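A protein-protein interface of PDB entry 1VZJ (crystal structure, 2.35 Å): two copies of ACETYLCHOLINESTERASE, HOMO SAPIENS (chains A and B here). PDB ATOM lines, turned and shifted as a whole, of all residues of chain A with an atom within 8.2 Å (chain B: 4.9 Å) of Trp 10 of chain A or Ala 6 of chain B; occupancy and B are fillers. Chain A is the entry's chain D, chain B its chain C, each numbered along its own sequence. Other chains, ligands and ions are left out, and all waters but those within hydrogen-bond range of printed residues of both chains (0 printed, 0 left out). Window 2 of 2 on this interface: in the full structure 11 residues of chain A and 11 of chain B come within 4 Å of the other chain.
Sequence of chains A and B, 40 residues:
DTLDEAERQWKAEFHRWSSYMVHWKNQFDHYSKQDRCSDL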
ATOM      1  N   LEU A   3      -3.540   1.057   4.657  1.00  0.00           N
ATOM      2  CA  LEU A   3      -4.373   2.237   4.559  1.00  0.00           C
ATOM      3  C   LEU A   3      -5.508   2.084   3.554  1.00  0.00           C
ATOM      4  O   LEU A   3      -6.639   2.512   3.836  1.00  0.00           O
ATOM      5  CB  LEU A   3      -3.536   3.476   4.243  1.00  0.00           C
ATOM      6  CG  LEU A   3      -2.632   3.969   5.391  1.00  0.00           C
ATOM      7  CD1 LEU A   3      -2.120   5.370   5.065  1.00  0.00           C
ATOM      8  CD2 LEU A   3      -3.429   3.998   6.695  1.00  0.00           C
ATOM      9  N   ASP A   4      -5.221   1.507   2.380  1.00  0.00           N
ATOM     10  CA  ASP A   4      -6.277   1.247   1.392  1.00  0.00           C
ATOM     11  C   ASP A   4      -7.278   0.352   2.102  1.00  0.00           C
ATOM     12  O   ASP A   4      -8.491   0.507   1.953  1.00  0.00           O
ATOM     13  CB  ASP A   4      -5.758   0.479   0.182  1.00  0.00           C
ATOM     14  CG  ASP A   4      -5.220   1.379  -0.896  1.00  0.00           C
ATOM     15  OD1 ASP A   4      -5.877   2.382  -1.239  1.00  0.00           O
ATOM     16  OD2 ASP A   4      -4.139   1.083  -1.425  1.00  0.00           O
ATOM     17  N   GLU A   5      -6.760  -0.587   2.882  1.00  0.00           N
ATOM     18  CA  GLU A   5      -7.596  -1.508   3.629  1.00  0.00           C
ATOM     19  C   GLU A   5      -8.423  -0.788   4.676  1.00  0.00           C
ATOM     20  O   GLU A   5      -9.561  -1.163   4.950  1.00  0.00           O
ATOM     21  CB  GLU A   5      -6.726  -2.539   4.321  1.00  0.00           C
ATOM     22  CG  GLU A   5      -7.484  -3.765   4.684  1.00  0.00           C
ATOM     23  CD  GLU A   5      -8.172  -4.359   3.460  1.00  0.00           C
ATOM     24  OE1 GLU A   5      -7.484  -4.554   2.420  1.00  0.00           O
ATOM     25  OE2 GLU A   5      -9.398  -4.624   3.549  1.00  0.00           O
ATOM     26  N   ALA A   6      -7.827   0.241   5.274  1.00  0.00           N
ATOM     27  CA  ALA A   6      -8.489   1.022   6.306  1.00  0.00           C
ATOM     28  C   ALA A   6      -9.556   1.852   5.638  1.00  0.00           C
ATOM     29  O   ALA A   6     -10.656   2.006   6.164  1.00  0.00           O
ATOM     30  CB  ALA A   6      -7.483   1.934   7.025  1.00  0.00           C
ATOM     31  N   GLU A   7      -9.227   2.389   4.473  1.00  0.00           N
ATOM     32  CA  GLU A   7     -10.181   3.193   3.737  1.00  0.00           C
ATOM     33  C   GLU A   7     -11.404   2.356   3.386  1.00  0.00           C
ATOM     34  O   GLU A   7     -12.538   2.778   3.582  1.00  0.00           O
ATOM     35  CB  GLU A   7      -9.546   3.728   2.463  1.00  0.00           C
ATOM     36  CG  GLU A   7     -10.445   4.642   1.688  1.00  0.00           C
ATOM     37  CD  GLU A   7      -9.742   5.235   0.493  1.00  0.00           C
ATOM     38  OE1 GLU A   7      -8.499   5.237   0.479  1.00  0.00           O
ATOM     39  OE2 GLU A   7     -10.422   5.718  -0.430  1.00  0.00           O
ATOM     40  N   ARG A   8     -11.149   1.153   2.887  1.00  0.00           N
ATOM     41  CA  ARG A   8     -12.192   0.228   2.490  1.00  0.00           C
ATOM     42  C   ARG A   8     -13.125  -0.093   3.639  1.00  0.00           C
ATOM     43  O   ARG A   8     -14.336   0.045   3.531  1.00  0.00           O
ATOM     44  CB  ARG A   8     -11.553  -1.071   1.993  1.00  0.00           C
ATOM     45  CG  ARG A   8     -12.492  -2.001   1.266  1.00  0.00           C
ATOM     46  CD  ARG A   8     -12.286  -3.453   1.678  1.00  0.00           C
ATOM     47  NE  ARG A   8     -13.331  -3.879   2.604  1.00  0.00           N
ATOM     48  CZ  ARG A   8     -13.114  -4.271   3.856  1.00  0.00           C
ATOM     49  NH1 ARG A   8     -11.875  -4.302   4.342  1.00  0.00           N
ATOM     50  NH2 ARG A   8     -14.139  -4.611   4.628  1.00  0.00           N
ATOM     51  N   GLN A   9     -12.548  -0.538   4.744  1.00  0.00           N
ATOM     52  CA  GLN A   9     -13.321  -0.930   5.917  1.00  0.00           C
ATOM     53  C   GLN A   9     -14.099   0.215   6.554  1.00  0.00           C
ATOM     54  O   GLN A   9     -15.150  -0.007   7.152  1.00  0.00           O
ATOM     55  CB  GLN A   9     -12.379  -1.560   6.934  1.00  0.00           C
ATOM     56  CG  GLN A   9     -13.014  -2.051   8.201  1.00  0.00           C
ATOM     57  CD  GLN A   9     -11.962  -2.274   9.294  1.00  0.00           C
ATOM     58  OE1 GLN A   9     -10.906  -2.871   9.039  1.00  0.00           O
ATOM     59  NE2 GLN A   9     -12.244  -1.797  10.511  1.00  0.00           N
ATOM     60  N   TRP A  10     -13.590   1.438   6.421  1.00  0.00           N
ATOM     61  CA  TRP A  10     -14.262   2.599   6.996  1.00  0.00           C
ATOM     62  C   TRP A  10     -15.474   2.961   6.153  1.00  0.00           C
ATOM     63  O   TRP A  10     -16.576   3.132   6.680  1.00  0.00           O
ATOM     64  CB  TRP A  10     -13.320   3.805   7.077  1.00  0.00           C
ATOM     65  CG  TRP A  10     -13.950   4.954   7.779  1.00  0.00           C
ATOM     66  CD1 TRP A  10     -14.078   5.117   9.126  1.00  0.00           C
ATOM     67  CD2 TRP A  10     -14.656   6.041   7.172  1.00  0.00           C
ATOM     68  NE1 TRP A  10     -14.831   6.235   9.402  1.00  0.00           N
ATOM     69  CE2 TRP A  10     -15.203   6.821   8.220  1.00  0.00           C
ATOM     70  CE3 TRP A  10     -14.895   6.426   5.849  1.00  0.00           C
ATOM     71  CZ2 TRP A  10     -15.969   7.989   7.976  1.00  0.00           C
ATOM     72  CZ3 TRP A  10     -15.658   7.585   5.609  1.00  0.00           C
ATOM     73  CH2 TRP A  10     -16.186   8.346   6.673  1.00  0.00           C
ATOM     74  N   LYS A  11     -15.267   3.079   4.841  1.00  0.00           N
ATOM     75  CA  LYS A  11     -16.350   3.402   3.916  1.00  0.00           C
ATOM     76  C   LYS A  11     -17.487   2.386   4.065  1.00  0.00           C
ATOM     77  O   LYS A  11     -18.665   2.737   4.120  1.00  0.00           O
ATOM     78  CB  LYS A  11     -15.822   3.410   2.480  1.00  0.00           C
ATOM     79  CG  LYS A  11     -14.925   4.609   2.177  1.00  0.00           C
ATOM     80  CD  LYS A  11     -14.524   4.701   0.704  1.00  0.00           C
ATOM     81  CE  LYS A  11     -13.814   6.052   0.419  1.00  0.00           C
ATOM     82  NZ  LYS A  11     -13.332   6.214  -0.998  1.00  0.00           N
ATOM     83  N   ALA A  12     -17.118   1.117   4.150  1.00  0.00           N
ATOM     84  CA  ALA A  12     -18.094   0.056   4.303  1.00  0.00           C
ATOM     85  C   ALA A  12     -18.867   0.183   5.613  1.00  0.00           C
ATOM     86  O   ALA A  12     -20.090   0.096   5.622  1.00  0.00           O
ATOM     87  CB  ALA A  12     -17.393  -1.311   4.235  1.00  0.00           C
ATOM     88  N   GLU A  13     -18.159   0.366   6.725  1.00  0.00           N
ATOM     89  CA  GLU A  13     -18.836   0.483   8.015  1.00  0.00           C
ATOM     90  C   GLU A  13     -19.667   1.761   8.134  1.00  0.00           C
ATOM     91  O   GLU A  13     -20.723   1.759   8.772  1.00  0.00           O
ATOM     92  CB  GLU A  13     -17.829   0.410   9.164  1.00  0.00           C
ATOM     93  CG  GLU A  13     -17.150  -0.933   9.267  1.00  0.00           C
ATOM     94  CD  GLU A  13     -16.308  -1.080  10.515  1.00  0.00           C
ATOM     95  OE1 GLU A  13     -15.365  -0.278  10.729  1.00  0.00           O
ATOM     96  OE2 GLU A  13     -16.592  -2.020  11.286  1.00  0.00           O
ATOM     97  N   PHE A  14     -19.187   2.838   7.517  1.00  0.00           N
ATOM     98  CA  PHE A  14     -19.878   4.122   7.533  1.00  0.00           C
ATOM     99  C   PHE A  14     -21.249   3.926   6.920  1.00  0.00           C
ATOM    100  O   PHE A  14     -22.281   4.076   7.580  1.00  0.00           O
ATOM    101  CB  PHE A  14     -19.108   5.131   6.690  1.00  0.00           C
ATOM    102  CG  PHE A  14     -19.636   6.535   6.770  1.00  0.00           C
ATOM    103  CD1 PHE A  14     -19.731   7.318   5.620  1.00  0.00           C
ATOM    104  CD2 PHE A  14     -19.957   7.108   7.995  1.00  0.00           C
ATOM    105  CE1 PHE A  14     -20.122   8.654   5.691  1.00  0.00           C
ATOM    106  CE2 PHE A  14     -20.350   8.440   8.078  1.00  0.00           C
ATOM    107  CZ  PHE A  14     -20.434   9.216   6.932  1.00  0.00           C
ATOM    108  N   HIS A  15     -21.235   3.605   5.633  1.00  0.00           N
ATOM    109  CA  HIS A  15     -22.438   3.364   4.861  1.00  0.00           C
ATOM    110  C   HIS A  15     -23.386   2.379   5.546  1.00  0.00           C
ATOM    111  O   HIS A  15     -24.598   2.531   5.478  1.00  0.00           O
ATOM    112  CB  HIS A  15     -22.044   2.861   3.460  1.00  0.00           C
ATOM    113  CG  HIS A  15     -21.477   3.929   2.573  1.00  0.00           C
ATOM    114  ND1 HIS A  15     -20.883   3.640   1.357  1.00  0.00           N
ATOM    115  CD2 HIS A  15     -21.446   5.269   2.702  1.00  0.00           C
ATOM    116  CE1 HIS A  15     -20.514   4.770   0.782  1.00  0.00           C
ATOM    117  NE2 HIS A  15     -20.841   5.774   1.572  1.00  0.00           N
ATOM    118  N   ARG A  16     -22.836   1.381   6.216  1.00  0.00           N
ATOM    119  CA  ARG A  16     -23.670   0.410   6.895  1.00  0.00           C
ATOM    120  C   ARG A  16     -24.307   1.084   8.094  1.00  0.00           C
ATOM    121  O   ARG A  16     -25.436   0.787   8.473  1.00  0.00           O
ATOM    122  CB  ARG A  16     -22.837  -0.784   7.345  1.00  0.00           C
ATOM    123  CG  ARG A  16     -23.640  -1.921   7.944  1.00  0.00           C
ATOM    124  CD  ARG A  16     -22.741  -3.113   8.275  1.00  0.00           C
ATOM    125  NE  ARG A  16     -23.502  -4.360   8.333  1.00  0.00           N
ATOM    126  CZ  ARG A  16     -23.715  -5.071   9.438  1.00  0.00           C
ATOM    127  NH1 ARG A  16     -23.224  -4.673  10.610  1.00  0.00           N
ATOM    128  NH2 ARG A  16     -24.432  -6.186   9.365  1.00  0.00           N
ATOM    129  N   TRP A  17     -23.561   2.005   8.689  1.00  0.00           N
ATOM    130  CA  TRP A  17     -24.039   2.764   9.835  1.00  0.00           C
ATOM    131  C   TRP A  17     -25.109   3.728   9.345  1.00  0.00           C
ATOM    132  O   TRP A  17     -26.193   3.818   9.933  1.00  0.00           O
ATOM    133  CB  TRP A  17     -22.888   3.547  10.456  1.00  0.00           C
ATOM    134  CG  TRP A  17     -23.300   4.450  11.567  1.00  0.00           C
ATOM    135  CD1 TRP A  17     -23.624   4.084  12.824  1.00  0.00           C
ATOM    136  CD2 TRP A  17     -23.418   5.873  11.514  1.00  0.00           C
ATOM    137  NE1 TRP A  17     -23.930   5.183  13.571  1.00  0.00           N
ATOM    138  CE2 TRP A  17     -23.808   6.301  12.788  1.00  0.00           C
ATOM    139  CE3 TRP A  17     -23.222   6.825  10.511  1.00  0.00           C
ATOM    140  CZ2 TRP A  17     -24.012   7.653  13.102  1.00  0.00           C
ATOM    141  CZ3 TRP A  17     -23.422   8.168  10.815  1.00  0.00           C
ATOM    142  CH2 TRP A  17     -23.811   8.569  12.106  1.00  0.00           C
ATOM    143  N   THR B   2      -8.829  12.656  -0.916  1.00  0.00           N
ATOM    144  CA  THR B   2      -9.843  11.626  -0.690  1.00  0.00           C
ATOM    145  C   THR B   2     -10.274  11.519   0.763  1.00  0.00           C
ATOM    146  O   THR B   2     -11.364  11.030   1.055  1.00  0.00           O
ATOM    147  CB  THR B   2      -9.344  10.242  -1.141  1.00  0.00           C
ATOM    148  OG1 THR B   2     -10.248   9.221  -0.692  1.00  0.00           O
ATOM    149  CG2 THR B   2      -7.984   9.968  -0.556  1.00  0.00           C
ATOM    150  N   LEU B   3      -9.416  11.961   1.675  1.00  0.00           N
ATOM    151  CA  LEU B   3      -9.729  11.912   3.094  1.00  0.00           C
ATOM    152  C   LEU B   3     -10.591  13.126   3.407  1.00  0.00           C
ATOM    153  O   LEU B   3     -11.569  13.033   4.145  1.00  0.00           O
ATOM    154  CB  LEU B   3      -8.450  11.971   3.923  1.00  0.00           C
ATOM    155  CG  LEU B   3      -8.437  11.367   5.332  1.00  0.00           C
ATOM    156  CD1 LEU B   3      -7.332  12.060   6.117  1.00  0.00           C
ATOM    157  CD2 LEU B   3      -9.763  11.537   6.036  1.00  0.00           C
ATOM    158  N   ASP B   4     -10.224  14.272   2.839  1.00  0.00           N
ATOM    159  CA  ASP B   4     -10.988  15.489   3.061  1.00  0.00           C
ATOM    160  C   ASP B   4     -12.417  15.187   2.707  1.00  0.00           C
ATOM    161  O   ASP B   4     -13.321  15.346   3.528  1.00  0.00           O
ATOM    162  CB  ASP B   4     -10.483  16.621   2.173  1.00  0.00           C
ATOM    163  CG  ASP B   4      -9.089  17.074   2.544  1.00  0.00           C
ATOM    164  OD1 ASP B   4      -8.736  16.998   3.738  1.00  0.00           O
ATOM    165  OD2 ASP B   4      -8.347  17.529   1.649  1.00  0.00           O
ATOM    166  N   GLU B   5     -12.623  14.737   1.475  1.00  0.00           N
ATOM    167  CA  GLU B   5     -13.956  14.415   0.996  1.00  0.00           C
ATOM    168  C   GLU B   5     -14.719  13.494   1.942  1.00  0.00           C
ATOM    169  O   GLU B   5     -15.914  13.688   2.181  1.00  0.00           O
ATOM    170  CB  GLU B   5     -13.895  13.775  -0.394  1.00  0.00           C
ATOM    171  CG  GLU B   5     -15.282  13.481  -0.972  1.00  0.00           C
ATOM    172  CD  GLU B   5     -16.160  14.733  -1.034  1.00  0.00           C
ATOM    173  OE1 GLU B   5     -16.236  15.477  -0.028  1.00  0.00           O
ATOM    174  OE2 GLU B   5     -16.787  14.967  -2.086  1.00  0.00           O
ATOM    175  N   ALA B   6     -14.034  12.490   2.478  1.00  0.00           N
ATOM    176  CA  ALA B   6     -14.677  11.564   3.393  1.00  0.00           C
ATOM    177  C   ALA B   6     -14.962  12.294   4.692  1.00  0.00           C
ATOM    178  O   ALA B   6     -15.958  12.031   5.373  1.00  0.00           O
ATOM    179  CB  ALA B   6     -13.786  10.362   3.640  1.00  0.00           C
ATOM    180  N   GLU B   7     -14.073  13.217   5.023  1.00  0.00           N
ATOM    181  CA  GLU B   7     -14.203  14.012   6.227  1.00  0.00           C
ATOM    182  C   GLU B   7     -15.473  14.858   6.065  1.00  0.00           C
ATOM    183  O   GLU B   7     -16.174  15.138   7.032  1.00  0.00           O
ATOM    184  CB  GLU B   7     -12.952  14.895   6.379  1.00  0.00           C
ATOM    185  CG  GLU B   7     -12.799  15.614   7.702  1.00  0.00           C
ATOM    186  CD  GLU B   7     -12.570  14.676   8.879  1.00  0.00           C
ATOM    187  OE1 GLU B   7     -11.492  14.036   8.941  1.00  0.00           O
ATOM    188  OE2 GLU B   7     -13.476  14.595   9.745  1.00  0.00           O
ATOM    189  N   ARG B   8     -15.773  15.233   4.827  1.00  0.00           N
ATOM    190  CA  ARG B   8     -16.954  16.035   4.530  1.00  0.00           C
ATOM    191  C   ARG B   8     -18.228  15.212   4.690  1.00  0.00           C
ATOM    192  O   ARG B   8     -19.192  15.650   5.329  1.00  0.00           O
ATOM    193  CB  ARG B   8     -16.873  16.585   3.106  1.00  0.00           C
ATOM    194  CG  ARG B   8     -17.867  17.702   2.794  1.00  0.00           C
ATOM    195  N   GLN B   9     -18.238  14.023   4.099  1.00  0.00           N
ATOM    196  CA  GLN B   9     -19.390  13.141   4.219  1.00  0.00           C
ATOM    197  C   GLN B   9     -19.671  12.872   5.685  1.00  0.00           C
ATOM    198  O   GLN B   9     -20.829  12.820   6.083  1.00  0.00           O
ATOM    199  CB  GLN B   9     -19.144  11.805   3.525  1.00  0.00           C
ATOM    200  CG  GLN B   9     -18.951  11.870   2.035  1.00  0.00           C
ATOM    201  CD  GLN B   9     -18.860  10.481   1.424  1.00  0.00           C
ATOM    202  OE1 GLN B   9     -18.094   9.627   1.888  1.00  0.00           O
ATOM    203  NE2 GLN B   9     -19.639  10.246   0.371  1.00  0.00           N
ATOM    204  N   TRP B  10     -18.610  12.683   6.479  1.00  0.00           N
ATOM    205  CA  TRP B  10     -18.743  12.414   7.915  1.00  0.00           C
ATOM    206  C   TRP B  10     -19.385  13.587   8.631  1.00  0.00           C
ATOM    207  O   TRP B  10     -20.274  13.406   9.462  1.00  0.00           O
ATOM    208  CB  TRP B  10     -17.385  12.157   8.579  1.00  0.00           C
ATOM    209  CG  TRP B  10     -17.533  11.810  10.057  1.00  0.00           C
ATOM    210  CD1 TRP B  10     -18.123  10.699  10.574  1.00  0.00           C
ATOM    211  CD2 TRP B  10     -17.122  12.600  11.186  1.00  0.00           C
ATOM    212  NE1 TRP B  10     -18.104  10.738  11.944  1.00  0.00           N
ATOM    213  CE2 TRP B  10     -17.491  11.893  12.345  1.00  0.00           C
ATOM    214  CE3 TRP B  10     -16.474  13.835  11.327  1.00  0.00           C
ATOM    215  CZ2 TRP B  10     -17.233  12.375  13.635  1.00  0.00           C
ATOM    216  CZ3 TRP B  10     -16.215  14.314  12.607  1.00  0.00           C
ATOM    217  CH2 TRP B  10     -16.592  13.583  13.744  1.00  0.00           C
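Printed residues of chain A that touch a printed residue of chain B: Glu 7, Trp 10 and Phe 14.
Hydrophobic or aromatic side chains of chain A that line the printed part of chain B: Trp 10 and Phe 14.
Hydrophobic or aromatic side chains of chain B within 4 Å of the printed part of chain A: Ala 6.
Along chain B the printed residues that touch a printed residue of chain A span positions 2 to 10.
Among the printed residues, 4 pairs touch across the chains.
Of chain B, only Ala 6 comes within 4 Å of Trp 10 of chain A.
Of chain A, only Trp 10 comes within 4 Å of Ala 6 of chain B.
Printed residues of chain B within 4 Å of Phe 14 of chain A: Gln 9 (3.7 Å) and Trp 10 (3.7 Å).
Printed residues of chain A within 4 Å of Trp 10 of chain B: Phe 14 (3.7 Å).
Printed residues of chain A within 4 Å of Gln 9 of chain B: Phe 14 (3.7 Å).
Printed residues of chain B within 4 Å of Glu 7 of chain A: Thr 2.
Leu 3 of chain A touches none of the printed residues of chain B.
Leu 3 of chain B touches none of the printed residues of chain A.
The nearest residue of chain B that does not touch Trp 10 of chain A is Trp 10 of chain B (4.3 Å).
Trp 10 of chain A touches Ala 6 of chain B, but with the chains exchanged Ala 6 of chain A does not touch Trp 10 of chain B (12.3 Å).
Of the 4 pairs that touch across the chains among the printed residues, none has its exchanged pair printed and touching as well.
The side-chain carboxylate of Glu 7 of chain A lies within salt-bridge range of the side-chain amino group of Lys 11 of chain A (3.0 Å).
Among the printed residues, merely in contact across the chains: Glu 7 of chain A with Thr 2 of chain B (3.5 Å), Phe 14 of chain A with Gln 9 of chain B (3.7 Å), Phe 14 of chain A with Trp 10 of chain B (3.7 Å) and Trp 10 of chain A with Ala 6 of chain B (3.9 Å).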
